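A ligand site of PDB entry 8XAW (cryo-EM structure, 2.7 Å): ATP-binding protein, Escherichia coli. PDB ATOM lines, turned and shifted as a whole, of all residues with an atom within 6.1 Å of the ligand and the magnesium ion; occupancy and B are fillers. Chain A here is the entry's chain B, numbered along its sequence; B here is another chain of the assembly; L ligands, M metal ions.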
ATOM      1  N   GLY A 151      36.262 -28.905  15.890  1.00  0.00           N
ATOM      2  CA  GLY A 151      35.459 -30.086  16.110  1.00  0.00           C
ATOM      3  C   GLY A 151      35.720 -31.097  15.015  1.00  0.00           C
ATOM      4  O   GLY A 151      36.241 -30.726  13.968  1.00  0.00           O
ATOM      5  N   SER A 152      35.335 -32.356  15.226  1.00  0.00           N
ATOM      6  CA  SER A 152      35.597 -33.394  14.232  1.00  0.00           C
ATOM      7  C   SER A 152      34.750 -33.172  12.979  1.00  0.00           C
ATOM      8  O   SER A 152      33.930 -32.247  12.903  1.00  0.00           O
ATOM      9  CB  SER A 152      35.337 -34.769  14.829  1.00  0.00           C
ATOM     10  OG  SER A 152      35.928 -35.787  14.043  1.00  0.00           O
ATOM     11  N   THR A 153      34.954 -34.015  11.978  1.00  0.00           N
ATOM     12  CA  THR A 153      34.233 -33.876  10.726  1.00  0.00           C
ATOM     13  C   THR A 153      32.738 -34.153  10.926  1.00  0.00           C
ATOM     14  O   THR A 153      32.347 -34.986  11.747  1.00  0.00           O
ATOM     15  CB  THR A 153      34.852 -34.779   9.634  1.00  0.00           C
ATOM     16  OG1 THR A 153      34.581 -34.226   8.343  1.00  0.00           O
ATOM     17  CG2 THR A 153      34.363 -36.218   9.697  1.00  0.00           C
ATOM     18  N   GLY A 154      31.920 -33.356  10.249  1.00  0.00           N
ATOM     19  CA  GLY A 154      30.484 -33.456  10.379  1.00  0.00           C
ATOM     20  C   GLY A 154      29.907 -33.081  11.728  1.00  0.00           C
ATOM     21  O   GLY A 154      28.757 -33.411  12.011  1.00  0.00           O
ATOM     22  N   SER A 155      30.679 -32.391  12.580  1.00  0.00           N
ATOM     23  CA  SER A 155      30.173 -32.015  13.898  1.00  0.00           C
ATOM     24  C   SER A 155      29.144 -30.893  13.800  1.00  0.00           C
ATOM     25  O   SER A 155      28.207 -30.855  14.611  1.00  0.00           O
ATOM     26  CB  SER A 155      31.321 -31.603  14.811  1.00  0.00           C
ATOM     27  OG  SER A 155      32.351 -30.957  14.074  1.00  0.00           O
ATOM     28  N   GLY A 156      29.299 -29.985  12.845  1.00  0.00           N
ATOM     29  CA  GLY A 156      28.359 -28.892  12.687  1.00  0.00           C
ATOM     30  C   GLY A 156      29.025 -27.536  12.780  1.00  0.00           C
ATOM     31  O   GLY A 156      28.370 -26.550  13.159  1.00  0.00           O
ATOM     32  N   LYS A 157      30.323 -27.474  12.487  1.00  0.00           N
ATOM     33  CA  LYS A 157      31.053 -26.203  12.566  1.00  0.00           C
ATOM     34  C   LYS A 157      30.533 -25.196  11.551  1.00  0.00           C
ATOM     35  O   LYS A 157      30.408 -24.009  11.867  1.00  0.00           O
ATOM     36  CB  LYS A 157      32.542 -26.432  12.353  1.00  0.00           C
ATOM     37  CG  LYS A 157      33.121 -27.627  13.088  1.00  0.00           C
ATOM     38  CD  LYS A 157      34.633 -27.613  12.990  1.00  0.00           C
ATOM     39  CE  LYS A 157      35.106 -28.207  11.664  1.00  0.00           C
ATOM     40  NZ  LYS A 157      34.667 -29.612  11.497  1.00  0.00           N
ATOM     41  N   SER A 158      30.235 -25.650  10.340  1.00  0.00           N
ATOM     42  CA  SER A 158      29.761 -24.742   9.295  1.00  0.00           C
ATOM     43  C   SER A 158      28.383 -24.185   9.628  1.00  0.00           C
ATOM     44  O   SER A 158      28.116 -23.005   9.376  1.00  0.00           O
ATOM     45  CB  SER A 158      29.727 -25.465   7.954  1.00  0.00           C
ATOM     46  OG  SER A 158      31.004 -25.973   7.621  1.00  0.00           O
ATOM     47  N   HIS A 159      27.501 -25.018  10.190  1.00  0.00           N
ATOM     48  CA  HIS A 159      26.189 -24.537  10.603  1.00  0.00           C
ATOM     49  C   HIS A 159      26.301 -23.578  11.774  1.00  0.00           C
ATOM     50  O   HIS A 159      25.538 -22.604  11.868  1.00  0.00           O
ATOM     51  CB  HIS A 159      25.282 -25.711  10.953  1.00  0.00           C
ATOM     52  CG  HIS A 159      24.648 -26.363   9.761  1.00  0.00           C
ATOM     53  ND1 HIS A 159      25.370 -26.864   8.705  1.00  0.00           N
ATOM     54  CD2 HIS A 159      23.344 -26.594   9.468  1.00  0.00           C
ATOM     55  CE1 HIS A 159      24.545 -27.372   7.804  1.00  0.00           C
ATOM     56  NE2 HIS A 159      23.312 -27.221   8.249  1.00  0.00           N
ATOM     57  N   THR A 160      27.233 -23.854  12.699  1.00  0.00           N
ATOM     58  CA  THR A 160      27.459 -22.940  13.818  1.00  0.00           C
ATOM     59  C   THR A 160      28.014 -21.612  13.340  1.00  0.00           C
ATOM     60  O   THR A 160      27.589 -20.544  13.808  1.00  0.00           O
ATOM     61  CB  THR A 160      28.407 -23.602  14.825  1.00  0.00           C
ATOM     62  OG1 THR A 160      27.804 -24.790  15.340  1.00  0.00           O
ATOM     63  CG2 THR A 160      28.702 -22.656  15.987  1.00  0.00           C
ATOM     64  N   HIS A 190      34.333 -24.984   0.052  1.00  0.00           N
ATOM     65  CA  HIS A 190      33.444 -26.105  -0.230  1.00  0.00           C
ATOM     66  C   HIS A 190      32.098 -25.633  -0.774  1.00  0.00           C
ATOM     67  O   HIS A 190      31.225 -26.479  -1.005  1.00  0.00           O
ATOM     68  CB  HIS A 190      33.241 -26.966   1.019  1.00  0.00           C
ATOM     69  CG  HIS A 190      34.493 -27.665   1.463  1.00  0.00           C
ATOM     70  ND1 HIS A 190      35.365 -28.261   0.591  1.00  0.00           N
ATOM     71  CD2 HIS A 190      35.016 -27.854   2.698  1.00  0.00           C
ATOM     72  CE1 HIS A 190      36.366 -28.789   1.252  1.00  0.00           C
ATOM     73  NE2 HIS A 190      36.177 -28.557   2.543  1.00  0.00           N
ATOM     74  N   GLU A 192      29.452 -23.665   0.459  1.00  0.00           N
ATOM     75  CA  GLU A 192      28.332 -23.957   1.345  1.00  0.00           C
ATOM     76  C   GLU A 192      27.500 -22.741   1.699  1.00  0.00           C
ATOM     77  O   GLU A 192      26.284 -22.854   1.817  1.00  0.00           O
ATOM     78  CB  GLU A 192      28.842 -24.589   2.641  1.00  0.00           C
ATOM     79  CG  GLU A 192      30.024 -25.523   2.479  1.00  0.00           C
ATOM     80  CD  GLU A 192      30.875 -25.566   3.730  1.00  0.00           C
ATOM     81  OE1 GLU A 192      30.294 -25.656   4.822  1.00  0.00           O
ATOM     82  OE2 GLU A 192      32.112 -25.482   3.624  1.00  0.00           O
ATOM     83  N   TYR A 193      28.133 -21.587   1.866  1.00  0.00           N
ATOM     84  CA  TYR A 193      27.477 -20.430   2.464  1.00  0.00           C
ATOM     85  C   TYR A 193      26.684 -19.599   1.466  1.00  0.00           C
ATOM     86  O   TYR A 193      26.101 -18.586   1.852  1.00  0.00           O
ATOM     87  CB  TYR A 193      28.530 -19.545   3.149  1.00  0.00           C
ATOM     88  CG  TYR A 193      29.125 -20.192   4.378  1.00  0.00           C
ATOM     89  CD1 TYR A 193      28.463 -20.151   5.595  1.00  0.00           C
ATOM     90  CD2 TYR A 193      30.341 -20.838   4.308  1.00  0.00           C
ATOM     91  CE1 TYR A 193      29.008 -20.744   6.718  1.00  0.00           C
ATOM     92  CE2 TYR A 193      30.891 -21.436   5.419  1.00  0.00           C
ATOM     93  CZ  TYR A 193      30.216 -21.387   6.620  1.00  0.00           C
ATOM     94  OH  TYR A 193      30.771 -21.981   7.723  1.00  0.00           O
ATOM     95  N   GLU A 426      37.189 -20.705   6.840  1.00  0.00           N
ATOM     96  CA  GLU A 426      36.690 -22.072   6.893  1.00  0.00           C
ATOM     97  C   GLU A 426      37.768 -23.042   6.450  1.00  0.00           C
ATOM     98  O   GLU A 426      38.389 -22.853   5.403  1.00  0.00           O
ATOM     99  CB  GLU A 426      35.446 -22.222   6.020  1.00  0.00           C
ATOM    100  CG  GLU A 426      34.140 -22.070   6.786  1.00  0.00           C
ATOM    101  CD  GLU A 426      33.572 -23.399   7.244  1.00  0.00           C
ATOM    102  OE1 GLU A 426      34.089 -23.983   8.215  1.00  0.00           O
ATOM    103  OE2 GLU A 426      32.590 -23.869   6.618  1.00  0.00           O
ATOM    104  N   GLU A 427      37.967 -24.107   7.243  1.00  0.00           N
ATOM    105  CA  GLU A 427      39.017 -25.104   7.060  1.00  0.00           C
ATOM    106  C   GLU A 427      40.385 -24.437   6.916  1.00  0.00           C
ATOM    107  O   GLU A 427      41.035 -24.482   5.865  1.00  0.00           O
ATOM    108  CB  GLU A 427      38.720 -26.025   5.870  1.00  0.00           C
ATOM    109  CG  GLU A 427      37.266 -26.441   5.715  1.00  0.00           C
ATOM    110  CD  GLU A 427      36.919 -27.673   6.528  1.00  0.00           C
ATOM    111  OE1 GLU A 427      36.354 -27.514   7.633  1.00  0.00           O
ATOM    112  OE2 GLU A 427      37.204 -28.783   6.043  1.00  0.00           O
ATOM    113  N   GLN A 466      39.253 -28.537  11.753  1.00  0.00           N
ATOM    114  CA  GLN A 466      38.833 -29.819  12.309  1.00  0.00           C
ATOM    115  C   GLN A 466      39.641 -30.220  13.543  1.00  0.00           C
ATOM    116  O   GLN A 466      39.073 -30.747  14.502  1.00  0.00           O
ATOM    117  CB  GLN A 466      38.915 -30.901  11.237  1.00  0.00           C
ATOM    118  CG  GLN A 466      37.603 -31.123  10.515  1.00  0.00           C
ATOM    119  CD  GLN A 466      37.754 -31.186   9.017  1.00  0.00           C
ATOM    120  OE1 GLN A 466      38.863 -31.164   8.501  1.00  0.00           O
ATOM    121  NE2 GLN A 466      36.631 -31.276   8.307  1.00  0.00           N
ATOM    122  N   MET A 485      33.608 -28.119  19.284  1.00  0.00           N
ATOM    123  CA  MET A 485      32.631 -29.175  19.080  1.00  0.00           C
ATOM    124  C   MET A 485      33.297 -30.518  19.384  1.00  0.00           C
ATOM    125  O   MET A 485      34.329 -30.575  20.058  1.00  0.00           O
ATOM    126  CB  MET A 485      32.035 -29.107  17.669  1.00  0.00           C
ATOM    127  CG  MET A 485      31.950 -27.732  17.052  1.00  0.00           C
ATOM    128  SD  MET A 485      30.286 -27.059  17.190  1.00  0.00           S
ATOM    129  CE  MET A 485      29.383 -28.142  16.125  1.00  0.00           C
ATOM    130  N   GLU A 516      25.858 -33.998  16.906  1.00  0.00           N
ATOM    131  CA  GLU A 516      25.745 -32.867  15.994  1.00  0.00           C
ATOM    132  C   GLU A 516      24.984 -31.718  16.662  1.00  0.00           C
ATOM    133  O   GLU A 516      23.860 -31.891  17.123  1.00  0.00           O
ATOM    134  CB  GLU A 516      25.029 -33.296  14.718  1.00  0.00           C
ATOM    135  CG  GLU A 516      25.949 -33.800  13.630  1.00  0.00           C
ATOM    136  CD  GLU A 516      25.403 -35.038  12.947  1.00  0.00           C
ATOM    137  OE1 GLU A 516      24.476 -35.666  13.502  1.00  0.00           O
ATOM    138  OE2 GLU A 516      25.892 -35.377  11.851  1.00  0.00           O
ATOM    139  N   GLY A 517      25.615 -30.545  16.699  1.00  0.00           N
ATOM    140  CA  GLY A 517      24.970 -29.323  17.119  1.00  0.00           C
ATOM    141  C   GLY A 517      25.483 -28.728  18.413  1.00  0.00           C
ATOM    142  O   GLY A 517      25.343 -27.514  18.607  1.00  0.00           O
ATOM    143  N   GLU A 518      26.064 -29.519  19.301  1.00  0.00           N
ATOM    144  CA  GLU A 518      26.530 -28.976  20.568  1.00  0.00           C
ATOM    145  C   GLU A 518      28.015 -28.639  20.541  1.00  0.00           C
ATOM    146  O   GLU A 518      28.796 -29.208  19.778  1.00  0.00           O
ATOM    147  CB  GLU A 518      26.249 -29.902  21.752  1.00  0.00           C
ATOM    148  CG  GLU A 518      24.910 -30.588  21.729  1.00  0.00           C
ATOM    149  CD  GLU A 518      24.950 -31.978  22.312  1.00  0.00           C
ATOM    150  OE1 GLU A 518      25.516 -32.142  23.421  1.00  0.00           O
ATOM    151  OE2 GLU A 518      24.378 -32.894  21.700  1.00  0.00           O
ATOM    152  N   LYS A 533      23.778 -25.798  23.044  1.00  0.00           N
ATOM    153  CA  LYS A 533      23.185 -26.268  21.798  1.00  0.00           C
ATOM    154  C   LYS A 533      23.097 -25.100  20.831  1.00  0.00           C
ATOM    155  O   LYS A 533      22.326 -24.162  21.067  1.00  0.00           O
ATOM    156  CB  LYS A 533      21.795 -26.864  22.051  1.00  0.00           C
ATOM    157  CG  LYS A 533      21.394 -27.991  21.105  1.00  0.00           C
ATOM    158  CD  LYS A 533      21.519 -29.345  21.769  1.00  0.00           C
ATOM    159  CE  LYS A 533      20.406 -29.565  22.779  1.00  0.00           C
ATOM    160  NZ  LYS A 533      20.786 -30.587  23.791  1.00  0.00           N
ATOM    161  N   ILE A 534      23.863 -25.154  19.746  1.00  0.00           N
ATOM    162  CA  ILE A 534      23.798 -24.110  18.734  1.00  0.00           C
ATOM    163  C   ILE A 534      22.465 -24.188  18.017  1.00  0.00           C
ATOM    164  O   ILE A 534      21.973 -25.279  17.688  1.00  0.00           O
ATOM    165  CB  ILE A 534      24.984 -24.233  17.758  1.00  0.00           C
ATOM    166  CG1 ILE A 534      26.297 -24.382  18.533  1.00  0.00           C
ATOM    167  CG2 ILE A 534      25.050 -23.031  16.824  1.00  0.00           C
ATOM    168  CD1 ILE A 534      26.749 -23.117  19.235  1.00  0.00           C
ATOM    169  N   GLU A 535      21.857 -23.024  17.778  1.00  0.00           N
ATOM    170  CA  GLU A 535      20.513 -22.963  17.233  1.00  0.00           C
ATOM    171  C   GLU A 535      20.477 -23.484  15.797  1.00  0.00           C
ATOM    172  O   GLU A 535      21.399 -23.233  15.012  1.00  0.00           O
ATOM    173  CB  GLU A 535      19.993 -21.519  17.304  1.00  0.00           C
ATOM    174  CG  GLU A 535      18.685 -21.252  16.586  1.00  0.00           C
ATOM    175  CD  GLU A 535      18.191 -19.835  16.800  1.00  0.00           C
ATOM    176  OE1 GLU A 535      18.877 -19.057  17.503  1.00  0.00           O
ATOM    177  OE2 GLU A 535      17.121 -19.483  16.254  1.00  0.00           O
ATOM    178  N   LYS A 536      19.423 -24.234  15.475  1.00  0.00           N
ATOM    179  CA  LYS A 536      19.248 -24.788  14.141  1.00  0.00           C
ATOM    180  C   LYS A 536      19.145 -23.701  13.089  1.00  0.00           C
ATOM    181  O   LYS A 536      18.518 -22.664  13.295  1.00  0.00           O
ATOM    182  CB  LYS A 536      17.990 -25.669  14.101  1.00  0.00           C
ATOM    183  CG  LYS A 536      17.928 -26.627  12.923  1.00  0.00           C
ATOM    184  CD  LYS A 536      19.157 -27.492  12.821  1.00  0.00           C
ATOM    185  CE  LYS A 536      18.777 -28.962  12.735  1.00  0.00           C
ATOM    186  NZ  LYS A 536      17.487 -29.167  12.022  1.00  0.00           N
ATOM    187  N   CYS A 537      19.788 -23.943  11.942  1.00  0.00           N
ATOM    188  CA  CYS A 537      19.741 -23.023  10.820  1.00  0.00           C
ATOM    189  C   CYS A 537      18.486 -23.297   9.996  1.00  0.00           C
ATOM    190  O   CYS A 537      18.368 -24.351   9.381  1.00  0.00           O
ATOM    191  CB  CYS A 537      21.000 -23.174   9.963  1.00  0.00           C
ATOM    192  SG  CYS A 537      22.327 -22.019  10.349  1.00  0.00           S
ATOM    193  N   SER A 543      25.740 -28.453   3.188  1.00  0.00           N
ATOM    194  CA  SER A 543      26.646 -29.446   3.737  1.00  0.00           C
ATOM    195  C   SER A 543      25.851 -30.602   4.314  1.00  0.00           C
ATOM    196  O   SER A 543      26.163 -31.130   5.390  1.00  0.00           O
ATOM    197  CB  SER A 543      27.576 -28.836   4.787  1.00  0.00           C
ATOM    198  OG  SER A 543      26.834 -28.262   5.853  1.00  0.00           O
ATOM    199  N   ILE A 544      24.794 -31.004   3.600  1.00  0.00           N
ATOM    200  CA  ILE A 544      23.933 -32.092   4.043  1.00  0.00           C
ATOM    201  C   ILE A 544      24.692 -33.403   3.978  1.00  0.00           C
ATOM    202  O   ILE A 544      25.370 -33.701   2.989  1.00  0.00           O
ATOM    203  CB  ILE A 544      22.645 -32.116   3.190  1.00  0.00           C
ATOM    204  CG1 ILE A 544      21.868 -33.420   3.407  1.00  0.00           C
ATOM    205  CG2 ILE A 544      22.966 -31.904   1.709  1.00  0.00           C
ATOM    206  CD1 ILE A 544      20.506 -33.423   2.745  1.00  0.00           C
ATOM    207  N   ASP A 545      24.617 -34.174   5.058  1.00  0.00           N
ATOM    208  CA  ASP A 545      25.317 -35.453   5.135  1.00  0.00           C
ATOM    209  C   ASP A 545      24.745 -36.441   4.125  1.00  0.00           C
ATOM    210  O   ASP A 545      23.524 -36.561   3.985  1.00  0.00           O
ATOM    211  CB  ASP A 545      25.227 -36.021   6.552  1.00  0.00           C
ATOM    212  CG  ASP A 545      26.465 -35.725   7.377  1.00  0.00           C
ATOM    213  OD1 ASP A 545      27.591 -35.901   6.856  1.00  0.00           O
ATOM    214  OD2 ASP A 545      26.314 -35.312   8.548  1.00  0.00           O
ATOM    215  N   ARG B 141      25.301 -43.480   9.013  1.00  0.00           N
ATOM    216  CA  ARG B 141      26.321 -42.951   9.903  1.00  0.00           C
ATOM    217  C   ARG B 141      27.543 -43.860  10.004  1.00  0.00           C
ATOM    218  O   ARG B 141      28.614 -43.398  10.414  1.00  0.00           O
ATOM    219  CB  ARG B 141      25.745 -42.708  11.292  1.00  0.00           C
ATOM    220  CG  ARG B 141      24.684 -41.620  11.335  1.00  0.00           C
ATOM    221  CD  ARG B 141      24.160 -41.410  12.765  1.00  0.00           C
ATOM    222  NE  ARG B 141      23.495 -40.120  12.979  1.00  0.00           N
ATOM    223  CZ  ARG B 141      24.043 -38.909  12.831  1.00  0.00           C
ATOM    224  NH1 ARG B 141      25.331 -38.759  12.586  1.00  0.00           N
ATOM    225  NH2 ARG B 141      23.279 -37.841  12.982  1.00  0.00           N
ATOM    226  N   LYS B 452      39.533 -35.391   5.822  1.00  0.00           N
ATOM    227  CA  LYS B 452      39.031 -34.080   6.232  1.00  0.00           C
ATOM    228  C   LYS B 452      37.799 -33.660   5.444  1.00  0.00           C
ATOM    229  O   LYS B 452      36.748 -33.385   6.032  1.00  0.00           O
ATOM    230  CB  LYS B 452      40.130 -33.033   6.103  1.00  0.00           C
ATOM    231  CG  LYS B 452      41.462 -33.402   6.711  1.00  0.00           C
ATOM    232  CD  LYS B 452      41.523 -33.013   8.164  1.00  0.00           C
ATOM    233  CE  LYS B 452      42.279 -31.715   8.322  1.00  0.00           C
ATOM    234  NZ  LYS B 452      43.606 -31.784   7.657  1.00  0.00           N
ATOM    235  N   GLU B 453      37.908 -33.607   4.124  1.00  0.00           N
ATOM    236  CA  GLU B 453      36.868 -33.008   3.298  1.00  0.00           C
ATOM    237  C   GLU B 453      36.137 -33.993   2.407  1.00  0.00           C
ATOM    238  O   GLU B 453      35.286 -33.562   1.615  1.00  0.00           O
ATOM    239  CB  GLU B 453      37.466 -31.879   2.450  1.00  0.00           C
ATOM    240  CG  GLU B 453      38.924 -32.076   2.082  1.00  0.00           C
ATOM    241  CD  GLU B 453      39.570 -30.819   1.537  1.00  0.00           C
ATOM    242  OE1 GLU B 453      40.544 -30.336   2.138  1.00  0.00           O
ATOM    243  OE2 GLU B 453      39.104 -30.318   0.482  1.00  0.00           O
ATOM    244  N   ARG B 455      33.934 -36.200   3.303  1.00  0.00           N
ATOM    245  CA  ARG B 455      32.593 -36.509   3.807  1.00  0.00           C
ATOM    246  C   ARG B 455      31.510 -35.896   2.935  1.00  0.00           C
ATOM    247  O   ARG B 455      30.492 -36.542   2.646  1.00  0.00           O
ATOM    248  CB  ARG B 455      32.454 -36.004   5.243  1.00  0.00           C
ATOM    249  CG  ARG B 455      31.406 -36.718   6.075  1.00  0.00           C
ATOM    250  CD  ARG B 455      31.045 -36.023   7.390  1.00  0.00           C
ATOM    251  NE  ARG B 455      30.054 -34.960   7.250  1.00  0.00           N
ATOM    252  CZ  ARG B 455      30.304 -33.710   6.865  1.00  0.00           C
ATOM    253  NH1 ARG B 455      31.537 -33.267   6.685  1.00  0.00           N
ATOM    254  NH2 ARG B 455      29.289 -32.875   6.692  1.00  0.00           N
ATOM    255  N   LYS B 456      31.702 -34.654   2.499  1.00  0.00           N
ATOM    256  CA  LYS B 456      30.694 -33.926   1.750  1.00  0.00           C
ATOM    257  C   LYS B 456      30.728 -34.208   0.254  1.00  0.00           C
ATOM    258  O   LYS B 456      29.847 -33.731  -0.471  1.00  0.00           O
ATOM    259  CB  LYS B 456      30.849 -32.424   1.993  1.00  0.00           C
ATOM    260  CG  LYS B 456      32.249 -31.899   1.726  1.00  0.00           C
ATOM    261  CD  LYS B 456      32.400 -30.475   2.218  1.00  0.00           C
ATOM    262  CE  LYS B 456      32.470 -30.433   3.741  1.00  0.00           C
ATOM    263  NZ  LYS B 456      31.628 -29.351   4.304  1.00  0.00           N
HETATM  264  P1  LIG L   1      33.239 -30.605   7.764  1.00  0.00           P
HETATM  265  O1  LIG L   1      33.436 -29.429   6.872  1.00  0.00           O
HETATM  266  O2  LIG L   1      34.200 -30.495   9.014  1.00  0.00           O
HETATM  267  O3  LIG L   1      33.577 -31.933   6.970  1.00  0.00           O
HETATM  268  P2  LIG L   1      31.397 -29.457   9.427  1.00  0.00           P
HETATM  269  O4  LIG L   1      31.677 -28.119   8.812  1.00  0.00           O
HETATM  270  O5  LIG L   1      32.370 -29.699  10.620  1.00  0.00           O
HETATM  271  N1  LIG L   1      31.631 -30.663   8.300  1.00  0.00           N
HETATM  272  P3  LIG L   1      28.680 -29.406   9.028  1.00  0.00           P
HETATM  273  O6  LIG L   1      29.084 -29.494   7.607  1.00  0.00           O
HETATM  274  O7  LIG L   1      27.931 -28.119   9.391  1.00  0.00           O
HETATM  275  O8  LIG L   1      29.939 -29.476   9.984  1.00  0.00           O
HETATM  276  O9  LIG L   1      27.821 -30.676   9.387  1.00  0.00           O
HETATM  277  C1  LIG L   1      26.573 -30.930   8.727  1.00  0.00           C
HETATM  278  C2  LIG L   1      25.713 -31.823   9.590  1.00  0.00           C
HETATM  279  O10 LIG L   1      25.645 -31.272  10.927  1.00  0.00           O
HETATM  280  C3  LIG L   1      24.272 -32.003   9.112  1.00  0.00           C
HETATM  281  O11 LIG L   1      23.866 -33.364   9.237  1.00  0.00           O
HETATM  282  C4  LIG L   1      23.486 -31.079  10.038  1.00  0.00           C
HETATM  283  O12 LIG L   1      22.149 -31.539  10.235  1.00  0.00           O
HETATM  284  C5  LIG L   1      24.292 -31.209  11.333  1.00  0.00           C
HETATM  285  N2  LIG L   1      24.126 -30.072  12.230  1.00  0.00           N
HETATM  286  C6  LIG L   1      24.873 -28.928  12.273  1.00  0.00           C
HETATM  287  N3  LIG L   1      24.496 -28.070  13.189  1.00  0.00           N
HETATM  288  C7  LIG L   1      23.425 -28.701  13.806  1.00  0.00           C
HETATM  289  C8  LIG L   1      22.572 -28.306  14.860  1.00  0.00           C
HETATM  290  N4  LIG L   1      22.684 -27.159  15.514  1.00  0.00           N
HETATM  291  N5  LIG L   1      21.602 -29.174  15.227  1.00  0.00           N
HETATM  292  C9  LIG L   1      21.493 -30.335  14.580  1.00  0.00           C
HETATM  293  N6  LIG L   1      22.230 -30.799  13.563  1.00  0.00           N
HETATM  294  C10 LIG L   1      23.186 -29.933  13.224  1.00  0.00           C
HETATM  295 MG    MG M   1      32.520 -27.269   7.127  1.00  0.00          MG
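Merely in contact with the magnesium ion: Glu 192, Glu 426, Glu 427 and Lys 456 of chain B.
Five residues have an atom within 4 Å of the magnesium ion: Ser 158, Glu 192, Glu 426, Glu 427 and Lys 456 of chain B.
The backbone NH (N) of Ile 534 is in hydrogen-bond range of the backbone carbonyl oxygen (O) of Gly 517.
The side-chain carboxylate of Glu 516 is in salt-bridge range of the guanidinium group of Arg 141 of chain B (2.5 Å).
NE of Arg 455 of chain B lies within salt-bridge range of OD1 of Asp 545.
OE2 of Glu 192 lies within salt-bridge range of NZ of Lys 456 of chain B, at 3.96 Å.
The backbone carbonyl oxygen (O) of Lys 452 of chain B is in hydrogen-bond range of the side-chain amide nitrogen (NE2) of Gln 466, at 3.1 Å.
The side-chain carboxylate of Glu 426 is in hydrogen-bond range of the side-chain hydroxyl of Tyr 193, 2.8 Å away.
The side-chain carboxylate (OE1) of Glu 192 sits close to the side-chain hydroxyl (OG) of Ser 158 (2.9 Å).
The side-chain hydroxyl (OG) of Ser 158 sits close to the side-chain carboxylate (OE2) of Glu 426 (2.8 Å).
The backbone NH of Gly 154 lies close to a nitrogen (N1) of the ligand (3.3 Å).
Ser 152 touches the ligand.
OG of Ser 155 touches O5 of the ligand, at 3.7 Å.
OE1 of Glu 427 touches O1 of the ligand, at 3.6 Å.
CG of Glu 516 touches O10 of the ligand, at 3.7 Å.
CA of Gly 517 touches C8 of the ligand, 3.4 Å away.
CE of Lys 536 touches C9 of the ligand (3.6 Å).
O of Lys 452 of chain B touches O3 of the ligand, 3.6 Å away.
Hydrophobic or aromatic side chains within 4 Å of the ligand: His 159.
Within 4 Å of the ligand: Ser 152, Thr 153, Gly 154, Ser 155, Gly 156, Lys 157, Ser 158, His 159, Glu 427, Gln 466, Glu 516, Gly 517, Ile 534, Lys 536, Ser 543, Asp 545, Lys 452 of chain B, Arg 455 of chain B and Lys 456 of chain B.
An oxygen (O1) of the ligand lies close to the side-chain amino group (NZ) of Lys 456 of chain B, 3.1 Å away.
An oxygen (O4) of the ligand sits close to the backbone NH (N) of Ser 158 (3.2 Å).
An oxygen (O5) of the ligand lies within salt-bridge range of the side-chain amino group of Lys 157 (2.5 Å).
NE2 of Gln 466 lies within hydrogen-bond range of O2 of the ligand (2.6 Å).
An oxygen (O7) of the ligand sits at hydrogen-bond distance from a ring nitrogen (ND1) of His 159 (2.9 Å).
The backbone NH of Gly 156 sits at hydrogen-bond distance from an oxygen (O8) of the ligand (3.0 Å).
NH1 of Arg 455 of chain B lies within salt-bridge range of O3 of the ligand.
An oxygen (O8) of the ligand is in hydrogen-bond range of the backbone NH (N) of Lys 157 (3.2 Å).
N of His 159 lies within hydrogen-bond range of O7 of the ligand (3.2 Å).
The backbone carbonyl oxygen of Ile 534 is in hydrogen-bond range of a nitrogen (N4) of the ligand (3.0 Å).
The side-chain carboxylate (OD2) of Asp 545 is in hydrogen-bond range of an oxygen (O11) of the ligand (3.2 Å).
The side-chain hydroxyl (OG1) of Thr 153 is in hydrogen-bond range of an oxygen (O3) of the ligand (2.9 Å).
O6 of the ligand is in hydrogen-bond range of OG of Ser 543 (3.1 Å).
The magnesium ion is bound by the side-chain hydroxyl of Ser 158, an oxygen (O4) of the ligand and an oxygen (O1) of the ligand.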
